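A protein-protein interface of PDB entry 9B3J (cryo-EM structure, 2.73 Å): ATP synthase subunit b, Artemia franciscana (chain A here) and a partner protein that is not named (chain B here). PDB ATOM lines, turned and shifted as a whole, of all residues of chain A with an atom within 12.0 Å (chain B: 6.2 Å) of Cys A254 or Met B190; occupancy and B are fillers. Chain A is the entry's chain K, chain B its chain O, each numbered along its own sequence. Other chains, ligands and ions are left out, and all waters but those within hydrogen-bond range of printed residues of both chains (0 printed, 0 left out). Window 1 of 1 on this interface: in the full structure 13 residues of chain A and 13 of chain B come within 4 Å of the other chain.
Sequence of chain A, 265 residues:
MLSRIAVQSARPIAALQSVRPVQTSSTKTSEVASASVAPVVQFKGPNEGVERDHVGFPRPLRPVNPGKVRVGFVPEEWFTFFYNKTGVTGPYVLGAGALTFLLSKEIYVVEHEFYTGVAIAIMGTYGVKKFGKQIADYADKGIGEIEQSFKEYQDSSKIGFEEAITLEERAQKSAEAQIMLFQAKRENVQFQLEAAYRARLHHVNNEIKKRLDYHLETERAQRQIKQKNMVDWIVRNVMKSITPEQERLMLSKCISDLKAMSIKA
OD2 of Asp A257 sits close to SD of Met B190, at 3.6 Å.
The backbone carbonyl oxygen (O) of Met A250 lies within hydrogen-bond range of the side-chain sulfur (SG) of Cys A254 (3.3 Å).
O of Val B181 lies within hydrogen-bond range of N of Val B188 (3.2 Å).
The backbone NH (N) of Leu B179 lies within hydrogen-bond range of the backbone carbonyl oxygen (O) of Met B190, 3.4 Å away.
The backbone carbonyl oxygen (O) of Gly B177 lies within hydrogen-bond range of the backbone NH (N) of Ile B192.
Among the printed residues, merely in contact across the chains: Met A250 with Ile B192 (3.7 Å), Cys A254 with Met B190 (3.8 Å) and Leu A258 with Val B181 (3.9 Å).
Cys A254 touches just one residue of chain B: Met B190.
Met B190 touches just these residues of chain A: Cys A254 (3.8 Å) and Asp A257 (3.6 Å).
No residue of chain A comes within 4 Å of Gly B178.
Leu B179 touches none of the printed residues of chain A.
Val B180 touches none of the printed residues of chain A.
No residue of chain A comes within 4 Å of Val B188.
No residue of chain A comes within 4 Å of Asp B189.
Printed residues of chain B within 4 Å of Asp A257: Met B190 (3.6 Å).
Of the printed residues of chain A, Val B181 touches Leu A258.
Leu A251 touches none of the printed residues of chain B.
Ile A263 touches none of the printed residues of chain B.
The nearest residue of chain B that does not touch Cys A254 is Gly B178 (5.0 Å).
The nearest printed residue of chain A that does not touch Val B181 is Cys A254 (6.8 Å).
Of the 12 printed residues of chain B, 3 touch a printed residue of chain A.
Hydrophobic or aromatic side chains of chain B that line the printed part of chain A: Val B181, Met B190 and Ile B192.
Of the 20 printed residues of chain A, 4 touch a printed residue of chain B.
Hydrophobic or aromatic side chains of chain A that line the printed part of chain B: Met A250 and Leu A258.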
ATOM      1  N   GLU A 245     -14.082 -25.331  -8.664  1.00  0.00           N
ATOM      2  CA  GLU A 245     -14.809 -24.347  -7.866  1.00  0.00           C
ATOM      3  C   GLU A 245     -15.267 -24.939  -6.537  1.00  0.00           C
ATOM      4  O   GLU A 245     -15.169 -24.284  -5.490  1.00  0.00           O
ATOM      5  CB  GLU A 245     -15.998 -23.793  -8.654  1.00  0.00           C
ATOM      6  CG  GLU A 245     -16.836 -24.832  -9.387  1.00  0.00           C
ATOM      7  CD  GLU A 245     -16.368 -25.064 -10.811  1.00  0.00           C
ATOM      8  OE1 GLU A 245     -15.479 -24.317 -11.273  1.00  0.00           O
ATOM      9  OE2 GLU A 245     -16.887 -25.992 -11.466  1.00  0.00           O
ATOM     10  N   GLN A 246     -15.747 -26.185  -6.553  1.00  0.00           N
ATOM     11  CA  GLN A 246     -16.120 -26.844  -5.308  1.00  0.00           C
ATOM     12  C   GLN A 246     -14.894 -27.190  -4.475  1.00  0.00           C
ATOM     13  O   GLN A 246     -14.972 -27.213  -3.243  1.00  0.00           O
ATOM     14  CB  GLN A 246     -16.945 -28.098  -5.601  1.00  0.00           C
ATOM     15  CG  GLN A 246     -17.710 -28.646  -4.407  1.00  0.00           C
ATOM     16  CD  GLN A 246     -18.691 -29.737  -4.793  1.00  0.00           C
ATOM     17  OE1 GLN A 246     -18.838 -30.068  -5.970  1.00  0.00           O
ATOM     18  NE2 GLN A 246     -19.371 -30.301  -3.801  1.00  0.00           N
ATOM     19  N   GLU A 247     -13.757 -27.450  -5.127  1.00  0.00           N
ATOM     20  CA  GLU A 247     -12.512 -27.665  -4.396  1.00  0.00           C
ATOM     21  C   GLU A 247     -12.076 -26.400  -3.663  1.00  0.00           C
ATOM     22  O   GLU A 247     -11.635 -26.466  -2.509  1.00  0.00           O
ATOM     23  CB  GLU A 247     -11.417 -28.132  -5.354  1.00  0.00           C
ATOM     24  CG  GLU A 247     -10.079 -28.397  -4.684  1.00  0.00           C
ATOM     25  CD  GLU A 247      -8.999 -28.787  -5.671  1.00  0.00           C
ATOM     26  OE1 GLU A 247      -9.302 -28.884  -6.878  1.00  0.00           O
ATOM     27  OE2 GLU A 247      -7.846 -28.996  -5.240  1.00  0.00           O
ATOM     28  N   ARG A 248     -12.200 -25.242  -4.316  1.00  0.00           N
ATOM     29  CA  ARG A 248     -11.894 -23.977  -3.653  1.00  0.00           C
ATOM     30  C   ARG A 248     -12.870 -23.697  -2.517  1.00  0.00           C
ATOM     31  O   ARG A 248     -12.476 -23.171  -1.468  1.00  0.00           O
ATOM     32  CB  ARG A 248     -11.912 -22.834  -4.664  1.00  0.00           C
ATOM     33  CG  ARG A 248     -10.813 -22.907  -5.706  1.00  0.00           C
ATOM     34  CD  ARG A 248     -10.984 -21.828  -6.762  1.00  0.00           C
ATOM     35  NE  ARG A 248      -9.986 -21.940  -7.818  1.00  0.00           N
ATOM     36  CZ  ARG A 248      -9.909 -21.132  -8.866  1.00  0.00           C
ATOM     37  NH1 ARG A 248     -10.761 -20.133  -9.032  1.00  0.00           N
ATOM     38  NH2 ARG A 248      -8.956 -21.331  -9.771  1.00  0.00           N
ATOM     39  N   LEU A 249     -14.150 -24.034  -2.714  1.00  0.00           N
ATOM     40  CA  LEU A 249     -15.137 -23.858  -1.649  1.00  0.00           C
ATOM     41  C   LEU A 249     -14.837 -24.753  -0.452  1.00  0.00           C
ATOM     42  O   LEU A 249     -14.970 -24.326   0.702  1.00  0.00           O
ATOM     43  CB  LEU A 249     -16.541 -24.135  -2.185  1.00  0.00           C
ATOM     44  CG  LEU A 249     -17.149 -23.080  -3.112  1.00  0.00           C
ATOM     45  CD1 LEU A 249     -18.507 -23.534  -3.624  1.00  0.00           C
ATOM     46  CD2 LEU A 249     -17.264 -21.740  -2.401  1.00  0.00           C
ATOM     47  N   MET A 250     -14.425 -25.998  -0.705  1.00  0.00           N
ATOM     48  CA  MET A 250     -14.091 -26.907   0.387  1.00  0.00           C
ATOM     49  C   MET A 250     -12.816 -26.476   1.100  1.00  0.00           C
ATOM     50  O   MET A 250     -12.711 -26.610   2.324  1.00  0.00           O
ATOM     51  CB  MET A 250     -13.958 -28.337  -0.135  1.00  0.00           C
ATOM     52  CG  MET A 250     -15.284 -28.980  -0.502  1.00  0.00           C
ATOM     53  SD  MET A 250     -15.119 -30.695  -1.024  1.00  0.00           S
ATOM     54  CE  MET A 250     -14.008 -30.515  -2.415  1.00  0.00           C
ATOM     55  N   LEU A 251     -11.837 -25.959   0.352  1.00  0.00           N
ATOM     56  CA  LEU A 251     -10.623 -25.440   0.976  1.00  0.00           C
ATOM     57  C   LEU A 251     -10.921 -24.222   1.840  1.00  0.00           C
ATOM     58  O   LEU A 251     -10.365 -24.081   2.937  1.00  0.00           O
ATOM     59  CB  LEU A 251      -9.585 -25.098  -0.091  1.00  0.00           C
ATOM     60  CG  LEU A 251      -8.452 -26.105  -0.287  1.00  0.00           C
ATOM     61  CD1 LEU A 251      -8.990 -27.452  -0.742  1.00  0.00           C
ATOM     62  CD2 LEU A 251      -7.428 -25.570  -1.274  1.00  0.00           C
ATOM     63  N   SER A 252     -11.799 -23.333   1.364  1.00  0.00           N
ATOM     64  CA  SER A 252     -12.194 -22.176   2.162  1.00  0.00           C
ATOM     65  C   SER A 252     -12.964 -22.597   3.406  1.00  0.00           C
ATOM     66  O   SER A 252     -12.802 -21.998   4.477  1.00  0.00           O
ATOM     67  CB  SER A 252     -13.030 -21.220   1.315  1.00  0.00           C
ATOM     68  OG  SER A 252     -14.225 -21.843   0.879  1.00  0.00           O
ATOM     69  N   LYS A 253     -13.806 -23.628   3.287  1.00  0.00           N
ATOM     70  CA  LYS A 253     -14.536 -24.128   4.449  1.00  0.00           C
ATOM     71  C   LYS A 253     -13.594 -24.775   5.460  1.00  0.00           C
ATOM     72  O   LYS A 253     -13.782 -24.624   6.672  1.00  0.00           O
ATOM     73  CB  LYS A 253     -15.614 -25.114   4.005  1.00  0.00           C
ATOM     74  CG  LYS A 253     -16.559 -25.535   5.117  1.00  0.00           C
ATOM     75  CD  LYS A 253     -17.747 -26.311   4.575  1.00  0.00           C
ATOM     76  CE  LYS A 253     -18.738 -26.643   5.680  1.00  0.00           C
ATOM     77  NZ  LYS A 253     -19.956 -27.311   5.150  1.00  0.00           N
ATOM     78  N   CYS A 254     -12.579 -25.499   4.981  1.00  0.00           N
ATOM     79  CA  CYS A 254     -11.588 -26.085   5.879  1.00  0.00           C
ATOM     80  C   CYS A 254     -10.770 -25.009   6.584  1.00  0.00           C
ATOM     81  O   CYS A 254     -10.449 -25.145   7.770  1.00  0.00           O
ATOM     82  CB  CYS A 254     -10.671 -27.034   5.109  1.00  0.00           C
ATOM     83  SG  CYS A 254     -11.458 -28.576   4.591  1.00  0.00           S
ATOM     84  N   ILE A 255     -10.421 -23.936   5.867  1.00  0.00           N
ATOM     85  CA  ILE A 255      -9.707 -22.820   6.482  1.00  0.00           C
ATOM     86  C   ILE A 255     -10.580 -22.135   7.529  1.00  0.00           C
ATOM     87  O   ILE A 255     -10.103 -21.769   8.611  1.00  0.00           O
ATOM     88  CB  ILE A 255      -9.224 -21.843   5.394  1.00  0.00           C
ATOM     89  CG1 ILE A 255      -8.080 -22.472   4.596  1.00  0.00           C
ATOM     90  CG2 ILE A 255      -8.772 -20.517   5.990  1.00  0.00           C
ATOM     91  CD1 ILE A 255      -7.558 -21.598   3.480  1.00  0.00           C
ATOM     92  N   SER A 256     -11.874 -21.971   7.234  1.00  0.00           N
ATOM     93  CA  SER A 256     -12.794 -21.378   8.202  1.00  0.00           C
ATOM     94  C   SER A 256     -12.954 -22.258   9.437  1.00  0.00           C
ATOM     95  O   SER A 256     -13.035 -21.750  10.560  1.00  0.00           O
ATOM     96  CB  SER A 256     -14.153 -21.129   7.550  1.00  0.00           C
ATOM     97  OG  SER A 256     -14.796 -22.352   7.241  1.00  0.00           O
ATOM     98  N   ASP A 257     -13.003 -23.580   9.249  1.00  0.00           N
ATOM     99  CA  ASP A 257     -13.079 -24.492  10.388  1.00  0.00           C
ATOM    100  C   ASP A 257     -11.797 -24.462  11.212  1.00  0.00           C
ATOM    101  O   ASP A 257     -11.844 -24.531  12.447  1.00  0.00           O
ATOM    102  CB  ASP A 257     -13.369 -25.913   9.905  1.00  0.00           C
ATOM    103  CG  ASP A 257     -14.741 -26.048   9.279  1.00  0.00           C
ATOM    104  OD1 ASP A 257     -15.648 -25.283   9.668  1.00  0.00           O
ATOM    105  OD2 ASP A 257     -14.911 -26.917   8.400  1.00  0.00           O
ATOM    106  N   LEU A 258     -10.644 -24.363  10.546  1.00  0.00           N
ATOM    107  CA  LEU A 258      -9.374 -24.242  11.257  1.00  0.00           C
ATOM    108  C   LEU A 258      -9.301 -22.935  12.037  1.00  0.00           C
ATOM    109  O   LEU A 258      -8.788 -22.902  13.161  1.00  0.00           O
ATOM    110  CB  LEU A 258      -8.215 -24.351  10.266  1.00  0.00           C
ATOM    111  CG  LEU A 258      -6.794 -24.270  10.822  1.00  0.00           C
ATOM    112  CD1 LEU A 258      -6.555 -25.358  11.853  1.00  0.00           C
ATOM    113  CD2 LEU A 258      -5.785 -24.374   9.693  1.00  0.00           C
ATOM    114  N   LYS A 259      -9.821 -21.850  11.460  1.00  0.00           N
ATOM    115  CA  LYS A 259      -9.868 -20.578  12.172  1.00  0.00           C
ATOM    116  C   LYS A 259     -10.836 -20.637  13.349  1.00  0.00           C
ATOM    117  O   LYS A 259     -10.580 -20.039  14.403  1.00  0.00           O
ATOM    118  CB  LYS A 259     -10.251 -19.451  11.211  1.00  0.00           C
ATOM    119  CG  LYS A 259     -10.066 -18.059  11.790  1.00  0.00           C
ATOM    120  CD  LYS A 259     -10.318 -16.984  10.746  1.00  0.00           C
ATOM    121  CE  LYS A 259     -10.033 -15.600  11.305  1.00  0.00           C
ATOM    122  NZ  LYS A 259     -10.206 -14.539  10.278  1.00  0.00           N
ATOM    123  N   ALA A 260     -11.953 -21.352  13.187  1.00  0.00           N
ATOM    124  CA  ALA A 260     -12.899 -21.521  14.286  1.00  0.00           C
ATOM    125  C   ALA A 260     -12.287 -22.331  15.422  1.00  0.00           C
ATOM    126  O   ALA A 260     -12.544 -22.050  16.599  1.00  0.00           O
ATOM    127  CB  ALA A 260     -14.180 -22.184  13.782  1.00  0.00           C
ATOM    128  N   MET A 261     -11.484 -23.344  15.089  1.00  0.00           N
ATOM    129  CA  MET A 261     -10.752 -24.071  16.121  1.00  0.00           C
ATOM    130  C   MET A 261      -9.677 -23.203  16.761  1.00  0.00           C
ATOM    131  O   MET A 261      -9.359 -23.384  17.943  1.00  0.00           O
ATOM    132  CB  MET A 261     -10.125 -25.338  15.539  1.00  0.00           C
ATOM    133  CG  MET A 261     -11.127 -26.410  15.159  1.00  0.00           C
ATOM    134  SD  MET A 261     -10.326 -27.959  14.709  1.00  0.00           S
ATOM    135  CE  MET A 261      -9.350 -27.447  13.299  1.00  0.00           C
ATOM    136  N   SER A 262      -9.096 -22.273  15.996  1.00  0.00           N
ATOM    137  CA  SER A 262      -8.128 -21.341  16.566  1.00  0.00           C
ATOM    138  C   SER A 262      -8.781 -20.391  17.559  1.00  0.00           C
ATOM    139  O   SER A 262      -8.150 -19.999  18.547  1.00  0.00           O
ATOM    140  CB  SER A 262      -7.438 -20.549  15.457  1.00  0.00           C
ATOM    141  OG  SER A 262      -8.298 -19.558  14.929  1.00  0.00           O
ATOM    142  N   ILE A 263     -10.033 -19.998  17.300  1.00  0.00           N
ATOM    143  CA  ILE A 263     -10.775 -19.179  18.256  1.00  0.00           C
ATOM    144  C   ILE A 263     -11.008 -19.947  19.551  1.00  0.00           C
ATOM    145  O   ILE A 263     -10.812 -19.418  20.652  1.00  0.00           O
ATOM    146  CB  ILE A 263     -12.100 -18.703  17.629  1.00  0.00           C
ATOM    147  CG1 ILE A 263     -11.821 -17.777  16.444  1.00  0.00           C
ATOM    148  CG2 ILE A 263     -12.972 -18.002  18.659  1.00  0.00           C
ATOM    149  CD1 ILE A 263     -13.070 -17.300  15.736  1.00  0.00           C
ATOM    150  N   LYS A 264     -11.405 -21.215  19.441  1.00  0.00           N
ATOM    151  CA  LYS A 264     -11.634 -22.063  20.610  1.00  0.00           C
ATOM    152  C   LYS A 264     -10.278 -22.483  21.172  1.00  0.00           C
ATOM    153  O   LYS A 264      -9.756 -23.567  20.901  1.00  0.00           O
ATOM    154  CB  LYS A 264     -12.488 -23.269  20.243  1.00  0.00           C
ATOM    155  CG  LYS A 264     -13.820 -22.917  19.609  1.00  0.00           C
ATOM    156  CD  LYS A 264     -14.579 -24.167  19.201  1.00  0.00           C
ATOM    157  CE  LYS A 264     -15.903 -23.821  18.543  1.00  0.00           C
ATOM    158  NZ  LYS A 264     -16.649 -25.041  18.130  1.00  0.00           N
ATOM    159  N   GLY B 177      -7.678 -34.341  -2.011  1.00  0.00           N
ATOM    160  CA  GLY B 177      -8.002 -32.956  -1.739  1.00  0.00           C
ATOM    161  C   GLY B 177      -7.943 -32.630  -0.263  1.00  0.00           C
ATOM    162  O   GLY B 177      -7.504 -33.455   0.544  1.00  0.00           O
ATOM    163  N   GLY B 178      -8.384 -31.432   0.106  1.00  0.00           N
ATOM    164  CA  GLY B 178      -8.412 -31.041   1.500  1.00  0.00           C
ATOM    165  C   GLY B 178      -7.101 -30.475   1.998  1.00  0.00           C
ATOM    166  O   GLY B 178      -6.325 -29.910   1.221  1.00  0.00           O
ATOM    167  N   LEU B 179      -6.843 -30.621   3.295  1.00  0.00           N
ATOM    168  CA  LEU B 179      -5.660 -30.043   3.912  1.00  0.00           C
ATOM    169  C   LEU B 179      -5.264 -30.879   5.118  1.00  0.00           C
ATOM    170  O   LEU B 179      -6.126 -31.383   5.843  1.00  0.00           O
ATOM    171  CB  LEU B 179      -5.915 -28.593   4.335  1.00  0.00           C
ATOM    172  CG  LEU B 179      -4.697 -27.676   4.391  1.00  0.00           C
ATOM    173  CD1 LEU B 179      -4.110 -27.520   3.002  1.00  0.00           C
ATOM    174  CD2 LEU B 179      -5.077 -26.325   4.971  1.00  0.00           C
ATOM    175  N   VAL B 180      -3.959 -31.020   5.331  1.00  0.00           N
ATOM    176  CA  VAL B 180      -3.414 -31.716   6.489  1.00  0.00           C
ATOM    177  C   VAL B 180      -2.630 -30.692   7.295  1.00  0.00           C
ATOM    178  O   VAL B 180      -1.597 -30.193   6.839  1.00  0.00           O
ATOM    179  CB  VAL B 180      -2.529 -32.902   6.087  1.00  0.00           C
ATOM    180  CG1 VAL B 180      -1.829 -33.476   7.302  1.00  0.00           C
ATOM    181  CG2 VAL B 180      -3.365 -33.970   5.407  1.00  0.00           C
ATOM    182  N   VAL B 181      -3.117 -30.375   8.491  1.00  0.00           N
ATOM    183  CA  VAL B 181      -2.532 -29.345   9.338  1.00  0.00           C
ATOM    184  C   VAL B 181      -2.033 -29.999  10.615  1.00  0.00           C
ATOM    185  O   VAL B 181      -2.780 -30.731  11.275  1.00  0.00           O
ATOM    186  CB  VAL B 181      -3.545 -28.230   9.658  1.00  0.00           C
ATOM    187  CG1 VAL B 181      -2.877 -27.114  10.442  1.00  0.00           C
ATOM    188  CG2 VAL B 181      -4.166 -27.694   8.381  1.00  0.00           C
ATOM    189  N   VAL B 188      -4.861 -32.328  13.079  1.00  0.00           N
ATOM    190  CA  VAL B 188      -6.193 -32.371  12.492  1.00  0.00           C
ATOM    191  C   VAL B 188      -6.063 -32.904  11.071  1.00  0.00           C
ATOM    192  O   VAL B 188      -5.210 -32.443  10.304  1.00  0.00           O
ATOM    193  CB  VAL B 188      -6.875 -30.987  12.525  1.00  0.00           C
ATOM    194  CG1 VAL B 188      -5.893 -29.883  12.147  1.00  0.00           C
ATOM    195  CG2 VAL B 188      -8.104 -30.957  11.631  1.00  0.00           C
ATOM    196  N   ASP B 189      -6.887 -33.892  10.730  1.00  0.00           N
ATOM    197  CA  ASP B 189      -6.841 -34.559   9.433  1.00  0.00           C
ATOM    198  C   ASP B 189      -8.050 -34.200   8.576  1.00  0.00           C
ATOM    199  O   ASP B 189      -8.620 -35.052   7.893  1.00  0.00           O
ATOM    200  CB  ASP B 189      -6.741 -36.072   9.605  1.00  0.00           C
ATOM    201  CG  ASP B 189      -7.777 -36.622  10.570  1.00  0.00           C
ATOM    202  OD1 ASP B 189      -8.500 -35.819  11.195  1.00  0.00           O
ATOM    203  OD2 ASP B 189      -7.866 -37.862  10.704  1.00  0.00           O
ATOM    204  N   MET B 190      -8.453 -32.930   8.605  1.00  0.00           N
ATOM    205  CA  MET B 190      -9.618 -32.464   7.851  1.00  0.00           C
ATOM    206  C   MET B 190      -9.230 -32.334   6.379  1.00  0.00           C
ATOM    207  O   MET B 190      -9.016 -31.244   5.844  1.00  0.00           O
ATOM    208  CB  MET B 190     -10.128 -31.145   8.419  1.00  0.00           C
ATOM    209  CG  MET B 190     -11.494 -30.730   7.903  1.00  0.00           C
ATOM    210  SD  MET B 190     -12.058 -29.176   8.620  1.00  0.00           S
ATOM    211  CE  MET B 190     -12.114 -29.605  10.357  1.00  0.00           C
ATOM    212  N   SER B 191      -9.144 -33.483   5.713  1.00  0.00           N
ATOM    213  CA  SER B 191      -8.813 -33.548   4.300  1.00  0.00           C
ATOM    214  C   SER B 191      -9.870 -34.371   3.577  1.00  0.00           C
ATOM    215  O   SER B 191     -10.552 -35.205   4.175  1.00  0.00           O
ATOM    216  CB  SER B 191      -7.422 -34.154   4.067  1.00  0.00           C
ATOM    217  OG  SER B 191      -7.373 -35.505   4.486  1.00  0.00           O
ATOM    218  N   ILE B 192      -9.995 -34.118   2.273  1.00  0.00           N
ATOM    219  CA  ILE B 192     -11.021 -34.786   1.476  1.00  0.00           C
ATOM    220  C   ILE B 192     -10.693 -36.264   1.302  1.00  0.00           C
ATOM    221  O   ILE B 192     -11.584 -37.123   1.375  1.00  0.00           O
ATOM    222  CB  ILE B 192     -11.184 -34.072   0.120  1.00  0.00           C
ATOM    223  CG1 ILE B 192     -11.541 -32.599   0.330  1.00  0.00           C
ATOM    224  CG2 ILE B 192     -12.243 -34.751  -0.734  1.00  0.00           C
ATOM    225  CD1 ILE B 192     -12.737 -32.373   1.228  1.00  0.00           C
ATOM    226  N   THR B 194      -8.880 -38.453   3.189  1.00  0.00           N
ATOM    227  CA  THR B 194      -9.133 -39.255   4.382  1.00  0.00           C
ATOM    228  C   THR B 194     -10.619 -39.317   4.714  1.00  0.00           C
ATOM    229  O   THR B 194     -11.096 -40.340   5.224  1.00  0.00           O
ATOM    230  CB  THR B 194      -8.354 -38.697   5.571  1.00  0.00           C
ATOM    231  OG1 THR B 194      -8.741 -37.336   5.800  1.00  0.00           O
ATOM    232  CG2 THR B 194      -6.860 -38.760   5.304  1.00  0.00           C
ATOM    233  N   LYS B 195     -11.360 -38.243   4.426  1.00  0.00           N
ATOM    234  CA  LYS B 195     -12.795 -38.222   4.701  1.00  0.00           C
ATOM    235  C   LYS B 195     -13.537 -39.234   3.835  1.00  0.00           C
ATOM    236  O   LYS B 195     -14.359 -40.015   4.336  1.00  0.00           O
ATOM    237  CB  LYS B 195     -13.348 -36.816   4.469  1.00  0.00           C
ATOM    238  CG  LYS B 195     -14.634 -36.520   5.212  1.00  0.00           C
ATOM    239  CD  LYS B 195     -14.372 -36.283   6.686  1.00  0.00           C
ATOM    240  CE  LYS B 195     -13.465 -35.080   6.889  1.00  0.00           C
ATOM    241  NZ  LYS B 195     -13.180 -34.829   8.328  1.00  0.00           N
